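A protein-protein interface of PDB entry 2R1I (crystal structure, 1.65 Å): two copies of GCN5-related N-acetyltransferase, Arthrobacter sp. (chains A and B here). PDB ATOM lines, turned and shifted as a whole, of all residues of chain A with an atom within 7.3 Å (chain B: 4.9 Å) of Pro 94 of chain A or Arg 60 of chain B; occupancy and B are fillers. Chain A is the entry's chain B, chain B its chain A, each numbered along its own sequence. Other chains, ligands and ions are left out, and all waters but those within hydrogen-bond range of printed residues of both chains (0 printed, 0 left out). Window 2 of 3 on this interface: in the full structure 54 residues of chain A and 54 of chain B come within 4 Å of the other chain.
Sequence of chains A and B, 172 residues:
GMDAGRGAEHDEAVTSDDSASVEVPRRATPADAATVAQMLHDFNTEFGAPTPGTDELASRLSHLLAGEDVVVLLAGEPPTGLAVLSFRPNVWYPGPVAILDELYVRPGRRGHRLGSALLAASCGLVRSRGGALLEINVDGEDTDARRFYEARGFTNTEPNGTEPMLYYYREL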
ATOM      1  N   PRO A  89      24.493 -19.652   8.044  1.00  0.00           N
ATOM      2  CA  PRO A  89      24.112 -19.520   6.652  1.00  0.00           C
ATOM      3  C   PRO A  89      22.660 -19.931   6.426  1.00  0.00           C
ATOM      4  O   PRO A  89      22.057 -20.530   7.310  1.00  0.00           O
ATOM      5  CB  PRO A  89      25.082 -20.468   5.911  1.00  0.00           C
ATOM      6  CG  PRO A  89      25.971 -21.040   6.935  1.00  0.00           C
ATOM      7  CD  PRO A  89      25.264 -20.873   8.256  1.00  0.00           C
ATOM      8  N   ASN A  90      22.135 -19.584   5.243  1.00  0.00           N
ATOM      9  CA  ASN A  90      20.758 -19.878   4.889  1.00  0.00           C
ATOM     10  C   ASN A  90      20.679 -20.045   3.384  1.00  0.00           C
ATOM     11  O   ASN A  90      21.349 -19.319   2.666  1.00  0.00           O
ATOM     12  CB  ASN A  90      19.868 -18.732   5.423  1.00  0.00           C
ATOM     13  CG  ASN A  90      18.396 -19.002   5.287  1.00  0.00           C
ATOM     14  OD1 ASN A  90      17.731 -19.396   6.249  1.00  0.00           O
ATOM     15  ND2 ASN A  90      17.895 -18.824   4.106  1.00  0.00           N
ATOM     16  N   VAL A  91      19.905 -21.019   2.900  1.00  0.00           N
ATOM     17  CA  VAL A  91      19.837 -21.290   1.438  1.00  0.00           C
ATOM     18  C   VAL A  91      19.310 -20.106   0.620  1.00  0.00           C
ATOM     19  O   VAL A  91      19.598 -19.985  -0.567  1.00  0.00           O
ATOM     20  CB  VAL A  91      19.085 -22.580   1.074  1.00  0.00           C
ATOM     21  CG1 VAL A  91      19.717 -23.807   1.743  1.00  0.00           C
ATOM     22  CG2 VAL A  91      17.552 -22.461   1.404  1.00  0.00           C
ATOM     23  N   TRP A  92      18.534 -19.210   1.257  1.00  0.00           N
ATOM     24  CA  TRP A  92      17.817 -18.137   0.556  1.00  0.00           C
ATOM     25  C   TRP A  92      18.558 -16.809   0.524  1.00  0.00           C
ATOM     26  O   TRP A  92      18.122 -15.876  -0.141  1.00  0.00           O
ATOM     27  CB  TRP A  92      16.411 -17.898   1.118  1.00  0.00           C
ATOM     28  CG  TRP A  92      15.567 -19.119   1.145  1.00  0.00           C
ATOM     29  CD1 TRP A  92      15.199 -19.752   2.231  1.00  0.00           C
ATOM     30  CD2 TRP A  92      15.040 -19.876   0.037  1.00  0.00           C
ATOM     31  NE1 TRP A  92      14.448 -20.832   1.937  1.00  0.00           N
ATOM     32  CE2 TRP A  92      14.311 -20.937   0.597  1.00  0.00           C
ATOM     33  CE3 TRP A  92      15.055 -19.733  -1.341  1.00  0.00           C
ATOM     34  CZ2 TRP A  92      13.689 -21.887  -0.166  1.00  0.00           C
ATOM     35  CZ3 TRP A  92      14.441 -20.674  -2.080  1.00  0.00           C
ATOM     36  CH2 TRP A  92      13.736 -21.720  -1.484  1.00  0.00           C
ATOM     37  N   TYR A  93      19.655 -16.694   1.250  1.00  0.00           N
ATOM     38  CA  TYR A  93      20.357 -15.402   1.350  1.00  0.00           C
ATOM     39  C   TYR A  93      21.846 -15.579   1.030  1.00  0.00           C
ATOM     40  O   TYR A  93      22.441 -16.605   1.349  1.00  0.00           O
ATOM     41  CB  TYR A  93      20.276 -14.816   2.771  1.00  0.00           C
ATOM     42  CG  TYR A  93      18.885 -14.497   3.257  1.00  0.00           C
ATOM     43  CD1 TYR A  93      18.315 -13.257   3.011  1.00  0.00           C
ATOM     44  CD2 TYR A  93      18.159 -15.414   3.981  1.00  0.00           C
ATOM     45  CE1 TYR A  93      17.036 -12.946   3.490  1.00  0.00           C
ATOM     46  CE2 TYR A  93      16.873 -15.133   4.434  1.00  0.00           C
ATOM     47  CZ  TYR A  93      16.317 -13.899   4.186  1.00  0.00           C
ATOM     48  OH  TYR A  93      15.043 -13.592   4.625  1.00  0.00           O
ATOM     49  N   PRO A  94      22.464 -14.531   0.444  1.00  0.00           N
ATOM     50  CA  PRO A  94      23.900 -14.555   0.250  1.00  0.00           C
ATOM     51  C   PRO A  94      24.691 -14.345   1.542  1.00  0.00           C
ATOM     52  O   PRO A  94      25.798 -14.848   1.656  1.00  0.00           O
ATOM     53  CB  PRO A  94      24.151 -13.410  -0.755  1.00  0.00           C
ATOM     54  CG  PRO A  94      23.012 -12.535  -0.648  1.00  0.00           C
ATOM     55  CD  PRO A  94      21.834 -13.322  -0.108  1.00  0.00           C
ATOM     56  N   GLY A  95      24.109 -13.629   2.494  1.00  0.00           N
ATOM     57  CA  GLY A  95      24.763 -13.370   3.769  1.00  0.00           C
ATOM     58  C   GLY A  95      24.186 -14.215   4.890  1.00  0.00           C
ATOM     59  O   GLY A  95      23.231 -14.975   4.667  1.00  0.00           O
ATOM     60  N   PRO A  96      24.763 -14.104   6.095  1.00  0.00           N
ATOM     61  CA  PRO A  96      24.228 -14.873   7.203  1.00  0.00           C
ATOM     62  C   PRO A  96      22.837 -14.389   7.658  1.00  0.00           C
ATOM     63  O   PRO A  96      22.411 -13.260   7.367  1.00  0.00           O
ATOM     64  CB  PRO A  96      25.256 -14.609   8.288  1.00  0.00           C
ATOM     65  CG  PRO A  96      25.782 -13.248   7.995  1.00  0.00           C
ATOM     66  CD  PRO A  96      25.860 -13.208   6.525  1.00  0.00           C
ATOM     67  N   ARG A 129      28.224  -7.573   8.361  1.00  0.00           N
ATOM     68  CA  ARG A 129      28.535  -8.965   7.995  1.00  0.00           C
ATOM     69  C   ARG A 129      27.767  -9.394   6.717  1.00  0.00           C
ATOM     70  O   ARG A 129      27.805 -10.550   6.351  1.00  0.00           O
ATOM     71  CB  ARG A 129      28.118  -9.888   9.151  1.00  0.00           C
ATOM     72  CG  ARG A 129      28.916  -9.811  10.476  1.00  0.00           C
ATOM     73  CD  ARG A 129      30.193 -10.585  10.417  1.00  0.00           C
ATOM     74  NE  ARG A 129      29.919 -12.010  10.274  1.00  0.00           N
ATOM     75  CZ  ARG A 129      29.848 -12.875  11.279  1.00  0.00           C
ATOM     76  NH1 ARG A 129      30.040 -12.495  12.521  1.00  0.00           N
ATOM     77  NH2 ARG A 129      29.566 -14.155  11.032  1.00  0.00           N
ATOM     78  N   GLY A 130      27.020  -8.477   6.115  1.00  0.00           N
ATOM     79  CA  GLY A 130      26.186  -8.757   4.968  1.00  0.00           C
ATOM     80  C   GLY A 130      24.856  -9.412   5.287  1.00  0.00           C
ATOM     81  O   GLY A 130      24.219 -10.008   4.404  1.00  0.00           O
ATOM     82  N   GLY A 131      24.460  -9.358   6.568  1.00  0.00           N
ATOM     83  CA  GLY A 131      23.221  -9.942   6.997  1.00  0.00           C
ATOM     84  C   GLY A 131      22.069  -9.012   6.739  1.00  0.00           C
ATOM     85  O   GLY A 131      22.190  -7.786   6.886  1.00  0.00           O
ATOM     86  N   ALA A 132      20.953  -9.579   6.290  1.00  0.00           N
ATOM     87  CA  ALA A 132      19.776  -8.788   5.989  1.00  0.00           C
ATOM     88  C   ALA A 132      18.579  -9.126   6.893  1.00  0.00           C
ATOM     89  O   ALA A 132      17.478  -8.622   6.712  1.00  0.00           O
ATOM     90  CB  ALA A 132      19.398  -8.944   4.514  1.00  0.00           C
ATOM     91  N   PRO B  52      15.020 -17.193  -5.625  1.00  0.00           N
ATOM     92  CA  PRO B  52      16.082 -16.918  -6.541  1.00  0.00           C
ATOM     93  C   PRO B  52      16.043 -17.940  -7.660  1.00  0.00           C
ATOM     94  O   PRO B  52      15.341 -18.948  -7.545  1.00  0.00           O
ATOM     95  CB  PRO B  52      17.363 -17.095  -5.704  1.00  0.00           C
ATOM     96  CG  PRO B  52      16.960 -17.210  -4.403  1.00  0.00           C
ATOM     97  CD  PRO B  52      15.517 -17.580  -4.311  1.00  0.00           C
ATOM     98  N   GLU B  56      21.681 -19.201  -9.135  1.00  0.00           N
ATOM     99  CA  GLU B  56      22.054 -18.631  -7.832  1.00  0.00           C
ATOM    100  C   GLU B  56      21.998 -19.673  -6.707  1.00  0.00           C
ATOM    101  O   GLU B  56      22.956 -19.796  -5.882  1.00  0.00           O
ATOM    102  CB  GLU B  56      21.194 -17.421  -7.458  1.00  0.00           C
ATOM    103  CG  GLU B  56      21.545 -16.829  -6.116  1.00  0.00           C
ATOM    104  CD  GLU B  56      20.621 -15.687  -5.686  1.00  0.00           C
ATOM    105  OE1 GLU B  56      20.069 -15.034  -6.590  1.00  0.00           O
ATOM    106  OE2 GLU B  56      20.424 -15.499  -4.428  1.00  0.00           O
ATOM    107  N   LEU B  57      20.896 -20.417  -6.667  1.00  0.00           N
ATOM    108  CA  LEU B  57      20.700 -21.432  -5.613  1.00  0.00           C
ATOM    109  C   LEU B  57      21.753 -22.522  -5.738  1.00  0.00           C
ATOM    110  O   LEU B  57      22.335 -22.937  -4.728  1.00  0.00           O
ATOM    111  CB  LEU B  57      19.273 -22.050  -5.673  1.00  0.00           C
ATOM    112  CG  LEU B  57      18.122 -21.161  -5.224  1.00  0.00           C
ATOM    113  CD1 LEU B  57      16.831 -21.826  -5.571  1.00  0.00           C
ATOM    114  CD2 LEU B  57      18.180 -20.861  -3.728  1.00  0.00           C
ATOM    115  N   ALA B  58      21.957 -23.022  -6.947  1.00  0.00           N
ATOM    116  CA  ALA B  58      22.960 -24.083  -7.190  1.00  0.00           C
ATOM    117  C   ALA B  58      24.366 -23.645  -6.762  1.00  0.00           C
ATOM    118  O   ALA B  58      25.079 -24.409  -6.177  1.00  0.00           O
ATOM    119  CB  ALA B  58      22.966 -24.539  -8.633  1.00  0.00           C
ATOM    120  N   SER B  59      24.736 -22.412  -7.095  1.00  0.00           N
ATOM    121  CA  SER B  59      26.036 -21.856  -6.730  1.00  0.00           C
ATOM    122  C   SER B  59      26.166 -21.787  -5.198  1.00  0.00           C
ATOM    123  O   SER B  59      27.191 -22.249  -4.627  1.00  0.00           O
ATOM    124  CB  SER B  59      26.224 -20.470  -7.360  1.00  0.00           C
ATOM    125  OG  SER B  59      27.369 -19.861  -6.793  1.00  0.00           O
ATOM    126  N   ARG B  60      25.128 -21.274  -4.524  1.00  0.00           N
ATOM    127  CA  ARG B  60      25.139 -21.214  -3.078  1.00  0.00           C
ATOM    128  C   ARG B  60      25.233 -22.608  -2.472  1.00  0.00           C
ATOM    129  O   ARG B  60      25.990 -22.867  -1.544  1.00  0.00           O
ATOM    130  CB  ARG B  60      23.918 -20.501  -2.531  1.00  0.00           C
ATOM    131  CG  ARG B  60      23.963 -20.277  -1.064  1.00  0.00           C
ATOM    132  CD  ARG B  60      23.491 -18.900  -0.719  1.00  0.00           C
ATOM    133  NE  ARG B  60      22.135 -18.683  -1.163  1.00  0.00           N
ATOM    134  CZ  ARG B  60      21.677 -17.671  -1.919  1.00  0.00           C
ATOM    135  NH1 ARG B  60      22.428 -16.670  -2.380  1.00  0.00           N
ATOM    136  NH2 ARG B  60      20.390 -17.654  -2.195  1.00  0.00           N
ATOM    137  N   LEU B  61      24.451 -23.527  -3.021  1.00  0.00           N
ATOM    138  CA  LEU B  61      24.436 -24.882  -2.494  1.00  0.00           C
ATOM    139  C   LEU B  61      25.753 -25.654  -2.719  1.00  0.00           C
ATOM    140  O   LEU B  61      26.091 -26.496  -1.913  1.00  0.00           O
ATOM    141  CB  LEU B  61      23.274 -25.654  -3.091  1.00  0.00           C
ATOM    142  CG  LEU B  61      21.924 -25.293  -2.474  1.00  0.00           C
ATOM    143  CD1 LEU B  61      20.904 -25.665  -3.497  1.00  0.00           C
ATOM    144  CD2 LEU B  61      21.684 -25.943  -1.095  1.00  0.00           C
ATOM    145  N   SER B  62      26.477 -25.345  -3.787  1.00  0.00           N
ATOM    146  CA  SER B  62      27.781 -25.961  -4.035  1.00  0.00           C
ATOM    147  C   SER B  62      28.752 -25.548  -2.950  1.00  0.00           C
ATOM    148  O   SER B  62      29.754 -26.238  -2.699  1.00  0.00           O
ATOM    149  CB  SER B  62      28.318 -25.570  -5.408  1.00  0.00           C
ATOM    150  OG  SER B  62      27.610 -26.262  -6.402  1.00  0.00           O
ATOM    151  N   HIS B  63      28.459 -24.413  -2.321  1.00  0.00           N
ATOM    152  CA  HIS B  63      29.173 -24.004  -1.124  1.00  0.00           C
ATOM    153  C   HIS B  63      28.666 -24.715   0.125  1.00  0.00           C
ATOM    154  O   HIS B  63      29.397 -25.432   0.781  1.00  0.00           O
ATOM    155  CB  HIS B  63      29.108 -22.491  -0.914  1.00  0.00           C
ATOM    156  CG  HIS B  63      30.132 -22.010   0.052  1.00  0.00           C
ATOM    157  ND1 HIS B  63      29.832 -21.479   1.292  1.00  0.00           N
ATOM    158  CD2 HIS B  63      31.480 -22.054  -0.028  1.00  0.00           C
ATOM    159  CE1 HIS B  63      30.961 -21.180   1.914  1.00  0.00           C
ATOM    160  NE2 HIS B  63      31.973 -21.554   1.151  1.00  0.00           N
ATOM    161  N   LEU B  64      27.393 -24.517   0.443  1.00  0.00           N
ATOM    162  CA  LEU B  64      26.810 -25.025   1.675  1.00  0.00           C
ATOM    163  C   LEU B  64      26.924 -26.541   1.826  1.00  0.00           C
ATOM    164  O   LEU B  64      27.220 -27.034   2.935  1.00  0.00           O
ATOM    165  CB  LEU B  64      25.355 -24.554   1.769  1.00  0.00           C
ATOM    166  CG  LEU B  64      25.160 -23.073   1.888  1.00  0.00           C
ATOM    167  CD1 LEU B  64      23.666 -22.711   1.879  1.00  0.00           C
ATOM    168  CD2 LEU B  64      25.869 -22.523   3.113  1.00  0.00           C
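The guanidinium group (NH1) of Arg 60 of chain B is in salt-bridge range of the side-chain carboxylate (OE2) of Glu 56 of chain B.
ND2 of Asn 90 of chain A lies close to N of Trp 92 of chain A (2.9 Å).
The guanidinium group of Arg 60 of chain B sits at hydrogen-bond distance from the backbone carbonyl oxygen of Val 91 of chain A, 2.9 Å away.
The guanidinium group (NE) of Arg 60 of chain B lies close to the backbone carbonyl oxygen (O) of Tyr 93 of chain A, 3.3 Å away.
No position is printed for both chains.
Printed residues of chain B within 4 Å of Pro 89 of chain A: Leu 64 (3.6 Å).
Printed residues of chain B within 4 Å of Asn 90 of chain A: Arg 60 (3.96 Å).
Of chain B, only Arg 60 (3.5 Å) comes within 4 Å of Pro 94 of chain A.
Leu 61 of chain B touches none of the printed residues of chain A.
Of the printed residues of chain A, Leu 64 of chain B touches Pro 89.
The nearest printed residue of chain B that does not touch Pro 94 of chain A is Glu 56 of chain B (5.0 Å).
The nearest residue of chain A that does not touch Arg 60 of chain B is Gly 95 of chain A (6.0 Å).
Pro 89 of chain A touches Leu 64 of chain B (CB to CD2, 3.6 Å).
Arg 60 of chain B touches Asn 90 of chain A.
O of Val 91 of chain A touches CD2 of Leu 57 of chain B, at 3.6 Å.
Pro 52 of chain B touches Trp 92 of chain A.
Arg 60 of chain B touches Trp 92 of chain A (NH2 to C, 3.4 Å).
Arg 60 of chain B touches Pro 94 of chain A.
Of the 12 printed residues of chain A, 6 touch a printed residue of chain B.
Printed residues of chain A that touch a printed residue of chain B: Pro 89, Asn 90, Val 91, Trp 92, Tyr 93 and Pro 94.
Along chain A the printed residues that touch a printed residue of chain B span positions 89 to 94.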
